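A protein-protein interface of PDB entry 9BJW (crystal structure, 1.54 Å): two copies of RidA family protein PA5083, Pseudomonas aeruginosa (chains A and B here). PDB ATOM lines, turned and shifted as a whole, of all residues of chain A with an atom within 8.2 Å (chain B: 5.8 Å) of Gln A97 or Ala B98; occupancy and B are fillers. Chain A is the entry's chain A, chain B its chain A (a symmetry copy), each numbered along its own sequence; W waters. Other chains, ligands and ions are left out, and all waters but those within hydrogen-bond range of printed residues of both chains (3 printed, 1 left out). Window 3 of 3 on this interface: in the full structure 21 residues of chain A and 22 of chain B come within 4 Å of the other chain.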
ATOM      1  N   THR A  64      14.922 -10.359  12.223  1.00  0.00           N
ATOM      2  CA  THR A  64      15.733 -10.941  13.286  1.00  0.00           C
ATOM      3  C   THR A  64      14.954 -12.121  13.850  1.00  0.00           C
ATOM      4  O   THR A  64      13.799 -11.971  14.274  1.00  0.00           O
ATOM      5  CB  THR A  64      16.088  -9.932  14.379  1.00  0.00           C
ATOM      6  OG1 THR A  64      16.878  -8.878  13.802  1.00  0.00           O
ATOM      7  CG2 THR A  64      16.923 -10.607  15.462  1.00  0.00           C
ATOM      8  N   ILE A  65      15.582 -13.291  13.833  1.00  0.00           N
ATOM      9  CA  ILE A  65      14.975 -14.539  14.277  1.00  0.00           C
ATOM     10  C   ILE A  65      15.646 -14.933  15.583  1.00  0.00           C
ATOM     11  O   ILE A  65      16.874 -15.075  15.633  1.00  0.00           O
ATOM     12  CB  ILE A  65      15.134 -15.648  13.222  1.00  0.00           C
ATOM     13  CG1 ILE A  65      14.500 -15.202  11.892  1.00  0.00           C
ATOM     14  CG2 ILE A  65      14.565 -16.975  13.728  1.00  0.00           C
ATOM     15  CD1 ILE A  65      14.702 -16.175  10.731  1.00  0.00           C
ATOM     16  N   TYR A  66      14.845 -15.101  16.634  1.00  0.00           N
ATOM     17  CA  TYR A  66      15.325 -15.496  17.957  1.00  0.00           C
ATOM     18  C   TYR A  66      14.916 -16.936  18.200  1.00  0.00           C
ATOM     19  O   TYR A  66      13.729 -17.265  18.104  1.00  0.00           O
ATOM     20  CB  TYR A  66      14.736 -14.602  19.055  1.00  0.00           C
ATOM     21  CG  TYR A  66      15.042 -13.131  18.894  1.00  0.00           C
ATOM     22  CD1 TYR A  66      16.237 -12.597  19.377  1.00  0.00           C
ATOM     23  CD2 TYR A  66      14.134 -12.273  18.273  1.00  0.00           C
ATOM     24  CE1 TYR A  66      16.533 -11.245  19.237  1.00  0.00           C
ATOM     25  CE2 TYR A  66      14.416 -10.923  18.127  1.00  0.00           C
ATOM     26  CZ  TYR A  66      15.617 -10.425  18.616  1.00  0.00           C
ATOM     27  OH  TYR A  66      15.898  -9.082  18.474  1.00  0.00           O
ATOM     28  N   LEU A  67      15.890 -17.788  18.508  1.00  0.00           N
ATOM     29  CA  LEU A  67      15.626 -19.181  18.847  1.00  0.00           C
ATOM     30  C   LEU A  67      16.009 -19.444  20.296  1.00  0.00           C
ATOM     31  O   LEU A  67      17.098 -19.055  20.734  1.00  0.00           O
ATOM     32  CB  LEU A  67      16.398 -20.117  17.906  1.00  0.00           C
ATOM     33  CG  LEU A  67      15.921 -20.133  16.454  1.00  0.00           C
ATOM     34  CD1 LEU A  67      16.921 -20.852  15.569  1.00  0.00           C
ATOM     35  CD2 LEU A  67      14.550 -20.796  16.369  1.00  0.00           C
ATOM     36  N   LYS A  68      15.119 -20.102  21.041  1.00  0.00           N
ATOM     37  CA  LYS A  68      15.457 -20.470  22.418  1.00  0.00           C
ATOM     38  C   LYS A  68      16.695 -21.358  22.458  1.00  0.00           C
ATOM     39  O   LYS A  68      17.537 -21.234  23.360  1.00  0.00           O
ATOM     40  CB  LYS A  68      14.277 -21.182  23.088  1.00  0.00           C
ATOM     41  CG  LYS A  68      14.518 -21.505  24.567  1.00  0.00           C
ATOM     42  CD  LYS A  68      13.395 -22.339  25.164  1.00  0.00           C
ATOM     43  CE  LYS A  68      13.498 -22.436  26.689  1.00  0.00           C
ATOM     44  NZ  LYS A  68      14.798 -23.031  27.127  1.00  0.00           N
ATOM     45  N   ASP A  69      16.813 -22.263  21.489  1.00  0.00           N
ATOM     46  CA  ASP A  69      17.888 -23.251  21.414  1.00  0.00           C
ATOM     47  C   ASP A  69      18.375 -23.301  19.967  1.00  0.00           C
ATOM     48  O   ASP A  69      17.844 -24.055  19.142  1.00  0.00           O
ATOM     49  CB  ASP A  69      17.403 -24.607  21.894  1.00  0.00           C
ATOM     50  CG  ASP A  69      18.538 -25.574  22.129  1.00  0.00           C
ATOM     51  OD1 ASP A  69      19.591 -25.428  21.473  1.00  0.00           O
ATOM     52  OD2 ASP A  69      18.377 -26.465  22.992  1.00  0.00           O
ATOM     53  N   ILE A  70      19.389 -22.495  19.657  1.00  0.00           N
ATOM     54  CA  ILE A  70      19.777 -22.345  18.262  1.00  0.00           C
ATOM     55  C   ILE A  70      20.435 -23.616  17.733  1.00  0.00           C
ATOM     56  O   ILE A  70      20.221 -23.989  16.576  1.00  0.00           O
ATOM     57  CB  ILE A  70      20.653 -21.092  18.058  1.00  0.00           C
ATOM     58  CG1 ILE A  70      20.844 -20.823  16.567  1.00  0.00           C
ATOM     59  CG2 ILE A  70      22.013 -21.208  18.747  1.00  0.00           C
ATOM     60  CD1 ILE A  70      21.160 -19.380  16.248  1.00  0.00           C
ATOM     61  N   ALA A  71      21.210 -24.320  18.565  1.00  0.00           N
ATOM     62  CA  ALA A  71      21.836 -25.551  18.087  1.00  0.00           C
ATOM     63  C   ALA A  71      20.786 -26.591  17.732  1.00  0.00           C
ATOM     64  O   ALA A  71      20.903 -27.300  16.723  1.00  0.00           O
ATOM     65  CB  ALA A  71      22.790 -26.098  19.151  1.00  0.00           C
ATOM     66  N   ARG A  72      19.732 -26.661  18.522  1.00  0.00           N
ATOM     67  CA  ARG A  72      18.740 -27.709  18.357  1.00  0.00           C
ATOM     68  C   ARG A  72      17.789 -27.420  17.206  1.00  0.00           C
ATOM     69  O   ARG A  72      17.375 -28.342  16.493  1.00  0.00           O
ATOM     70  CB  ARG A  72      17.947 -27.852  19.636  1.00  0.00           C
ATOM     71  CG  ARG A  72      17.021 -29.016  19.630  1.00  0.00           C
ATOM     72  CD  ARG A  72      16.684 -29.259  21.035  1.00  0.00           C
ATOM     73  NE  ARG A  72      15.787 -30.377  21.236  1.00  0.00           N
ATOM     74  CZ  ARG A  72      15.468 -30.802  22.444  1.00  0.00           C
ATOM     75  NH1 ARG A  72      15.967 -30.222  23.522  1.00  0.00           N
ATOM     76  NH2 ARG A  72      14.632 -31.827  22.574  1.00  0.00           N
ATOM     77  N   ASP A  73      17.434 -26.152  17.018  1.00  0.00           N
ATOM     78  CA  ASP A  73      16.292 -25.803  16.183  1.00  0.00           C
ATOM     79  C   ASP A  73      16.630 -25.019  14.924  1.00  0.00           C
ATOM     80  O   ASP A  73      15.708 -24.702  14.158  1.00  0.00           O
ATOM     81  CB  ASP A  73      15.269 -25.014  17.009  1.00  0.00           C
ATOM     82  CG  ASP A  73      14.567 -25.879  18.025  1.00  0.00           C
ATOM     83  OD1 ASP A  73      14.473 -27.102  17.778  1.00  0.00           O
ATOM     84  OD2 ASP A  73      14.119 -25.352  19.062  1.00  0.00           O
ATOM     85  N   THR A  94      19.054 -12.079  10.460  1.00  0.00           N
ATOM     86  CA  THR A  94      19.969 -12.370  11.551  1.00  0.00           C
ATOM     87  C   THR A  94      19.281 -13.392  12.439  1.00  0.00           C
ATOM     88  O   THR A  94      18.122 -13.200  12.809  1.00  0.00           O
ATOM     89  CB  THR A  94      20.282 -11.098  12.354  1.00  0.00           C
ATOM     90  OG1 THR A  94      20.860 -10.108  11.489  1.00  0.00           O
ATOM     91  CG2 THR A  94      21.213 -11.403  13.511  1.00  0.00           C
ATOM     92  N   THR A  95      19.975 -14.478  12.776  1.00  0.00           N
ATOM     93  CA  THR A  95      19.415 -15.532  13.608  1.00  0.00           C
ATOM     94  C   THR A  95      20.332 -15.729  14.811  1.00  0.00           C
ATOM     95  O   THR A  95      21.521 -16.027  14.647  1.00  0.00           O
ATOM     96  CB  THR A  95      19.247 -16.842  12.829  1.00  0.00           C
ATOM     97  OG1 THR A  95      18.498 -16.579  11.631  1.00  0.00           O
ATOM     98  CG2 THR A  95      18.505 -17.841  13.658  1.00  0.00           C
ATOM     99  N   VAL A  96      19.781 -15.565  16.015  1.00  0.00           N
ATOM    100  CA  VAL A  96      20.560 -15.683  17.244  1.00  0.00           C
ATOM    101  C   VAL A  96      19.749 -16.422  18.297  1.00  0.00           C
ATOM    102  O   VAL A  96      18.525 -16.568  18.192  1.00  0.00           O
ATOM    103  CB  VAL A  96      20.993 -14.306  17.800  1.00  0.00           C
ATOM    104  CG1 VAL A  96      21.732 -13.502  16.764  1.00  0.00           C
ATOM    105  CG2 VAL A  96      19.767 -13.545  18.369  1.00  0.00           C
ATOM    106  N   GLN A  97      20.444 -16.867  19.347  1.00  0.00           N
ATOM    107  CA  GLN A  97      19.800 -17.516  20.475  1.00  0.00           C
ATOM    108  C   GLN A  97      19.355 -16.492  21.518  1.00  0.00           C
ATOM    109  O   GLN A  97      20.126 -15.607  21.900  1.00  0.00           O
ATOM    110  CB  GLN A  97      20.751 -18.518  21.124  1.00  0.00           C
ATOM    111  CG  GLN A  97      20.132 -19.226  22.315  1.00  0.00           C
ATOM    112  CD  GLN A  97      20.891 -20.467  22.682  1.00  0.00           C
ATOM    113  OE1 GLN A  97      20.872 -21.457  21.957  1.00  0.00           O
ATOM    114  NE2 GLN A  97      21.601 -20.413  23.800  1.00  0.00           N
ATOM    115  N   ALA A  98      18.120 -16.635  21.997  1.00  0.00           N
ATOM    116  CA  ALA A  98      17.657 -15.864  23.139  1.00  0.00           C
ATOM    117  C   ALA A  98      16.441 -16.555  23.728  1.00  0.00           C
ATOM    118  O   ALA A  98      15.569 -17.015  22.985  1.00  0.00           O
ATOM    119  CB  ALA A  98      17.288 -14.434  22.737  1.00  0.00           C
ATOM    120  N   GLU A  99      16.367 -16.598  25.052  1.00  0.00           N
ATOM    121  CA  GLU A  99      15.137 -17.063  25.675  1.00  0.00           C
ATOM    122  C   GLU A  99      14.033 -16.034  25.468  1.00  0.00           C
ATOM    123  O   GLU A  99      14.269 -14.821  25.524  1.00  0.00           O
ATOM    124  CB  GLU A  99      15.349 -17.324  27.165  1.00  0.00           C
ATOM    125  CG  GLU A  99      14.115 -17.924  27.823  1.00  0.00           C
ATOM    126  CD  GLU A  99      14.451 -19.048  28.775  1.00  0.00           C
ATOM    127  OE1 GLU A  99      13.516 -19.614  29.382  1.00  0.00           O
ATOM    128  OE2 GLU A  99      15.649 -19.372  28.917  1.00  0.00           O
ATOM    129  N   LEU A 100      12.824 -16.517  25.200  1.00  0.00           N
ATOM    130  CA  LEU A 100      11.671 -15.654  25.010  1.00  0.00           C
ATOM    131  C   LEU A 100      10.869 -15.591  26.316  1.00  0.00           C
ATOM    132  O   LEU A 100      11.244 -16.175  27.334  1.00  0.00           O
ATOM    133  CB  LEU A 100      10.829 -16.131  23.822  1.00  0.00           C
ATOM    134  CG  LEU A 100      11.496 -16.154  22.430  1.00  0.00           C
ATOM    135  CD1 LEU A 100      12.404 -14.926  22.201  1.00  0.00           C
ATOM    136  CD2 LEU A 100      12.250 -17.470  22.142  1.00  0.00           C
ATOM    137  N   LEU A 106       9.706 -21.382  21.463  1.00  0.00           N
ATOM    138  CA  LEU A 106      10.976 -21.784  20.885  1.00  0.00           C
ATOM    139  C   LEU A 106      11.506 -20.797  19.864  1.00  0.00           C
ATOM    140  O   LEU A 106      12.703 -20.831  19.562  1.00  0.00           O
ATOM    141  CB  LEU A 106      10.854 -23.157  20.214  1.00  0.00           C
ATOM    142  CG  LEU A 106      10.292 -24.256  21.103  1.00  0.00           C
ATOM    143  CD1 LEU A 106      10.191 -25.551  20.304  1.00  0.00           C
ATOM    144  CD2 LEU A 106      11.166 -24.438  22.352  1.00  0.00           C
ATOM    145  N   TYR B  66      26.403  -8.916  18.524  1.00  0.00           N
ATOM    146  CA  TYR B  66      26.097 -10.101  19.324  1.00  0.00           C
ATOM    147  C   TYR B  66      27.403 -10.792  19.668  1.00  0.00           C
ATOM    148  O   TYR B  66      28.181 -11.122  18.767  1.00  0.00           O
ATOM    149  CB  TYR B  66      25.187 -11.071  18.562  1.00  0.00           C
ATOM    150  CG  TYR B  66      23.868 -10.478  18.125  1.00  0.00           C
ATOM    151  CD1 TYR B  66      22.777 -10.455  18.996  1.00  0.00           C
ATOM    152  CD2 TYR B  66      23.704  -9.954  16.843  1.00  0.00           C
ATOM    153  CE1 TYR B  66      21.557  -9.912  18.610  1.00  0.00           C
ATOM    154  CE2 TYR B  66      22.491  -9.411  16.445  1.00  0.00           C
ATOM    155  CZ  TYR B  66      21.428  -9.401  17.338  1.00  0.00           C
ATOM    156  OH  TYR B  66      20.221  -8.863  16.943  1.00  0.00           O
ATOM    157  N   LEU B  67      27.642 -11.004  20.959  1.00  0.00           N
ATOM    158  CA  LEU B  67      28.819 -11.731  21.421  1.00  0.00           C
ATOM    159  C   LEU B  67      28.394 -13.029  22.095  1.00  0.00           C
ATOM    160  O   LEU B  67      27.485 -13.029  22.932  1.00  0.00           O
ATOM    161  CB  LEU B  67      29.638 -10.865  22.388  1.00  0.00           C
ATOM    162  CG  LEU B  67      30.339  -9.659  21.761  1.00  0.00           C
ATOM    163  CD1 LEU B  67      30.865  -8.727  22.834  1.00  0.00           C
ATOM    164  CD2 LEU B  67      31.470 -10.133  20.855  1.00  0.00           C
ATOM    165  N   LYS B  68      29.049 -14.134  21.731  1.00  0.00           N
ATOM    166  CA  LYS B  68      28.757 -15.402  22.403  1.00  0.00           C
ATOM    167  C   LYS B  68      29.016 -15.300  23.901  1.00  0.00           C
ATOM    168  O   LYS B  68      28.270 -15.865  24.715  1.00  0.00           O
ATOM    169  CB  LYS B  68      29.596 -16.534  21.800  1.00  0.00           C
ATOM    170  CG  LYS B  68      29.269 -17.913  22.381  1.00  0.00           C
ATOM    171  CD  LYS B  68      30.215 -18.991  21.874  1.00  0.00           C
ATOM    172  CE  LYS B  68      29.733 -20.398  22.237  1.00  0.00           C
ATOM    173  NZ  LYS B  68      29.582 -20.576  23.713  1.00  0.00           N
ATOM    174  N   ASP B  69      30.076 -14.587  24.277  1.00  0.00           N
ATOM    175  CA  ASP B  69      30.524 -14.449  25.662  1.00  0.00           C
ATOM    176  C   ASP B  69      30.872 -12.980  25.894  1.00  0.00           C
ATOM    177  O   ASP B  69      32.008 -12.549  25.655  1.00  0.00           O
ATOM    178  CB  ASP B  69      31.705 -15.361  25.936  1.00  0.00           C
ATOM    179  CG  ASP B  69      32.005 -15.488  27.410  1.00  0.00           C
ATOM    180  OD1 ASP B  69      31.694 -14.542  28.165  1.00  0.00           O
ATOM    181  OD2 ASP B  69      32.532 -16.550  27.809  1.00  0.00           O
ATOM    182  N   VAL B  96      25.078  -7.041  22.962  1.00  0.00           N
ATOM    183  CA  VAL B  96      24.451  -7.986  23.881  1.00  0.00           C
ATOM    184  C   VAL B  96      25.038  -9.373  23.671  1.00  0.00           C
ATOM    185  O   VAL B  96      25.677  -9.662  22.653  1.00  0.00           O
ATOM    186  CB  VAL B  96      22.915  -8.044  23.707  1.00  0.00           C
ATOM    187  CG1 VAL B  96      22.296  -6.677  23.827  1.00  0.00           C
ATOM    188  CG2 VAL B  96      22.551  -8.739  22.369  1.00  0.00           C
ATOM    189  N   GLN B  97      24.785 -10.256  24.641  1.00  0.00           N
ATOM    190  CA  GLN B  97      25.203 -11.643  24.546  1.00  0.00           C
ATOM    191  C   GLN B  97      24.144 -12.489  23.841  1.00  0.00           C
ATOM    192  O   GLN B  97      22.955 -12.408  24.164  1.00  0.00           O
ATOM    193  CB  GLN B  97      25.463 -12.214  25.937  1.00  0.00           C
ATOM    194  CG  GLN B  97      25.899 -13.666  25.901  1.00  0.00           C
ATOM    195  CD  GLN B  97      26.535 -14.090  27.193  1.00  0.00           C
ATOM    196  OE1 GLN B  97      27.637 -13.664  27.524  1.00  0.00           O
ATOM    197  NE2 GLN B  97      25.827 -14.910  27.956  1.00  0.00           N
ATOM    198  N   ALA B  98      24.586 -13.321  22.898  1.00  0.00           N
ATOM    199  CA  ALA B  98      23.716 -14.327  22.308  1.00  0.00           C
ATOM    200  C   ALA B  98      24.580 -15.388  21.652  1.00  0.00           C
ATOM    201  O   ALA B  98      25.569 -15.060  20.991  1.00  0.00           O
ATOM    202  CB  ALA B  98      22.779 -13.712  21.265  1.00  0.00           C
ATOM    203  N   GLU B  99      24.190 -16.646  21.805  1.00  0.00           N
ATOM    204  CA  GLU B  99      24.854 -17.689  21.038  1.00  0.00           C
ATOM    205  C   GLU B  99      24.480 -17.564  19.566  1.00  0.00           C
ATOM    206  O   GLU B  99      23.332 -17.254  19.222  1.00  0.00           O
ATOM    207  CB  GLU B  99      24.482 -19.072  21.567  1.00  0.00           C
ATOM    208  CG  GLU B  99      25.250 -20.181  20.863  1.00  0.00           C
ATOM    209  CD  GLU B  99      25.751 -21.240  21.818  1.00  0.00           C
ATOM    210  OE1 GLU B  99      26.392 -22.207  21.353  1.00  0.00           O
ATOM    211  OE2 GLU B  99      25.510 -21.107  23.036  1.00  0.00           O
ATOM    212  N   LEU B 100      25.458 -17.779  18.693  1.00  0.00           N
ATOM    213  CA  LEU B 100      25.238 -17.724  17.257  1.00  0.00           C
ATOM    214  C   LEU B 100      25.049 -19.149  16.722  1.00  0.00           C
ATOM    215  O   LEU B 100      25.051 -20.127  17.472  1.00  0.00           O
ATOM    216  CB  LEU B 100      26.383 -16.980  16.563  1.00  0.00           C
ATOM    217  CG  LEU B 100      26.621 -15.503  16.950  1.00  0.00           C
ATOM    218  CD1 LEU B 100      25.295 -14.734  17.142  1.00  0.00           C
ATOM    219  CD2 LEU B 100      27.548 -15.338  18.173  1.00  0.00           C
HETATM  220  O   HOH W   1      18.400  -8.219  18.777  1.00  0.00           O
HETATM  221  O   HOH W   2      20.612 -14.008  24.194  1.00  0.00           O
HETATM  222  O   HOH W   3      19.502  -8.004  14.587  1.00  0.00           O
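N of Gln A97 sits at hydrogen-bond distance from O of Glu B99, at 2.9 Å.
O of Thr A94 is in hydrogen-bond range of N of Ile A65.
The backbone carbonyl oxygen (O) of Ile A65 lies within hydrogen-bond range of the backbone NH (N) of Val A96.
The backbone carbonyl oxygen (O) of Val A96 sits at hydrogen-bond distance from the backbone NH (N) of Leu A67, at 2.9 Å.
N of Ile A70 is in hydrogen-bond range of OE1 of Gln A97 (2.9 Å).
The backbone carbonyl oxygen (O) of Leu B67 lies within hydrogen-bond range of the backbone NH (N) of Ala B98, 2.9 Å away.
Leu B100 touches Ile A70.
Thr A94 touches Tyr B66.
Val A96 touches Tyr B66.
Val A96 touches Ala B98 (CB to CB, 3.9 Å).
Val A96 touches Glu B99 (CA to O, 3.8 Å).
CD1 of Leu B100 touches CG1 of Val A96 (3.8 Å).
Ala B98 touches Gln A97 (CB to O, 3.3 Å).
Of chain B, only Ala B98 and Glu B99 come within 4 Å of Gln A97.
Ala B98 touches just these residues of chain A: Val A96 (3.9 Å) and Gln A97 (3.3 Å).
Printed residues of chain B within 4 Å of Thr A94: Tyr B66 (3.8 Å).
Of the printed residues of chain A, Glu B99 touches Val A96 and Gln A97.
Printed residues of chain A within 4 Å of Leu B100: Ile A70 (3.5 Å) and Val A96 (3.8 Å).
Of the printed residues of chain A, Tyr B66 touches Thr A94 (3.8 Å) and Val A96 (3.9 Å).
Of the printed residues of chain B, Ile A70 touches Leu B100.
Printed residues of chain A that touch a printed residue of chain B: Ile A70, Thr A94, Val A96 and Gln A97.
Val A96 touches Tyr B66, but with the chains exchanged Tyr A66 does not touch Val B96 (7.2 Å).
Val A96 touches Glu B99, but with the chains exchanged Glu A99 does not touch Val B96 (10.4 Å).
Val A96 touches Leu B100, but with the chains exchanged Leu A100 does not touch Val B96 (11.9 Å).
Gln A97 touches Glu B99, but with the chains exchanged Glu A99 does not touch Gln B97 (7.9 Å).
Positions printed for both chains: 66, 67, 68, 69, 96, 97, 98, 99 and 100.
Water W3 bridges OH of Tyr B66 (2.6 Å) and OG1 of Thr A64 (2.9 Å).
Water W1 bridges the side-chain hydroxyl (OH) of Tyr B66 and the side-chain hydroxyl (OH) of Tyr A66.
Water W2 lies within hydrogen-bond range of O of Gln B97 (2.8 Å) and O of Gln A97 (2.8 Å).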
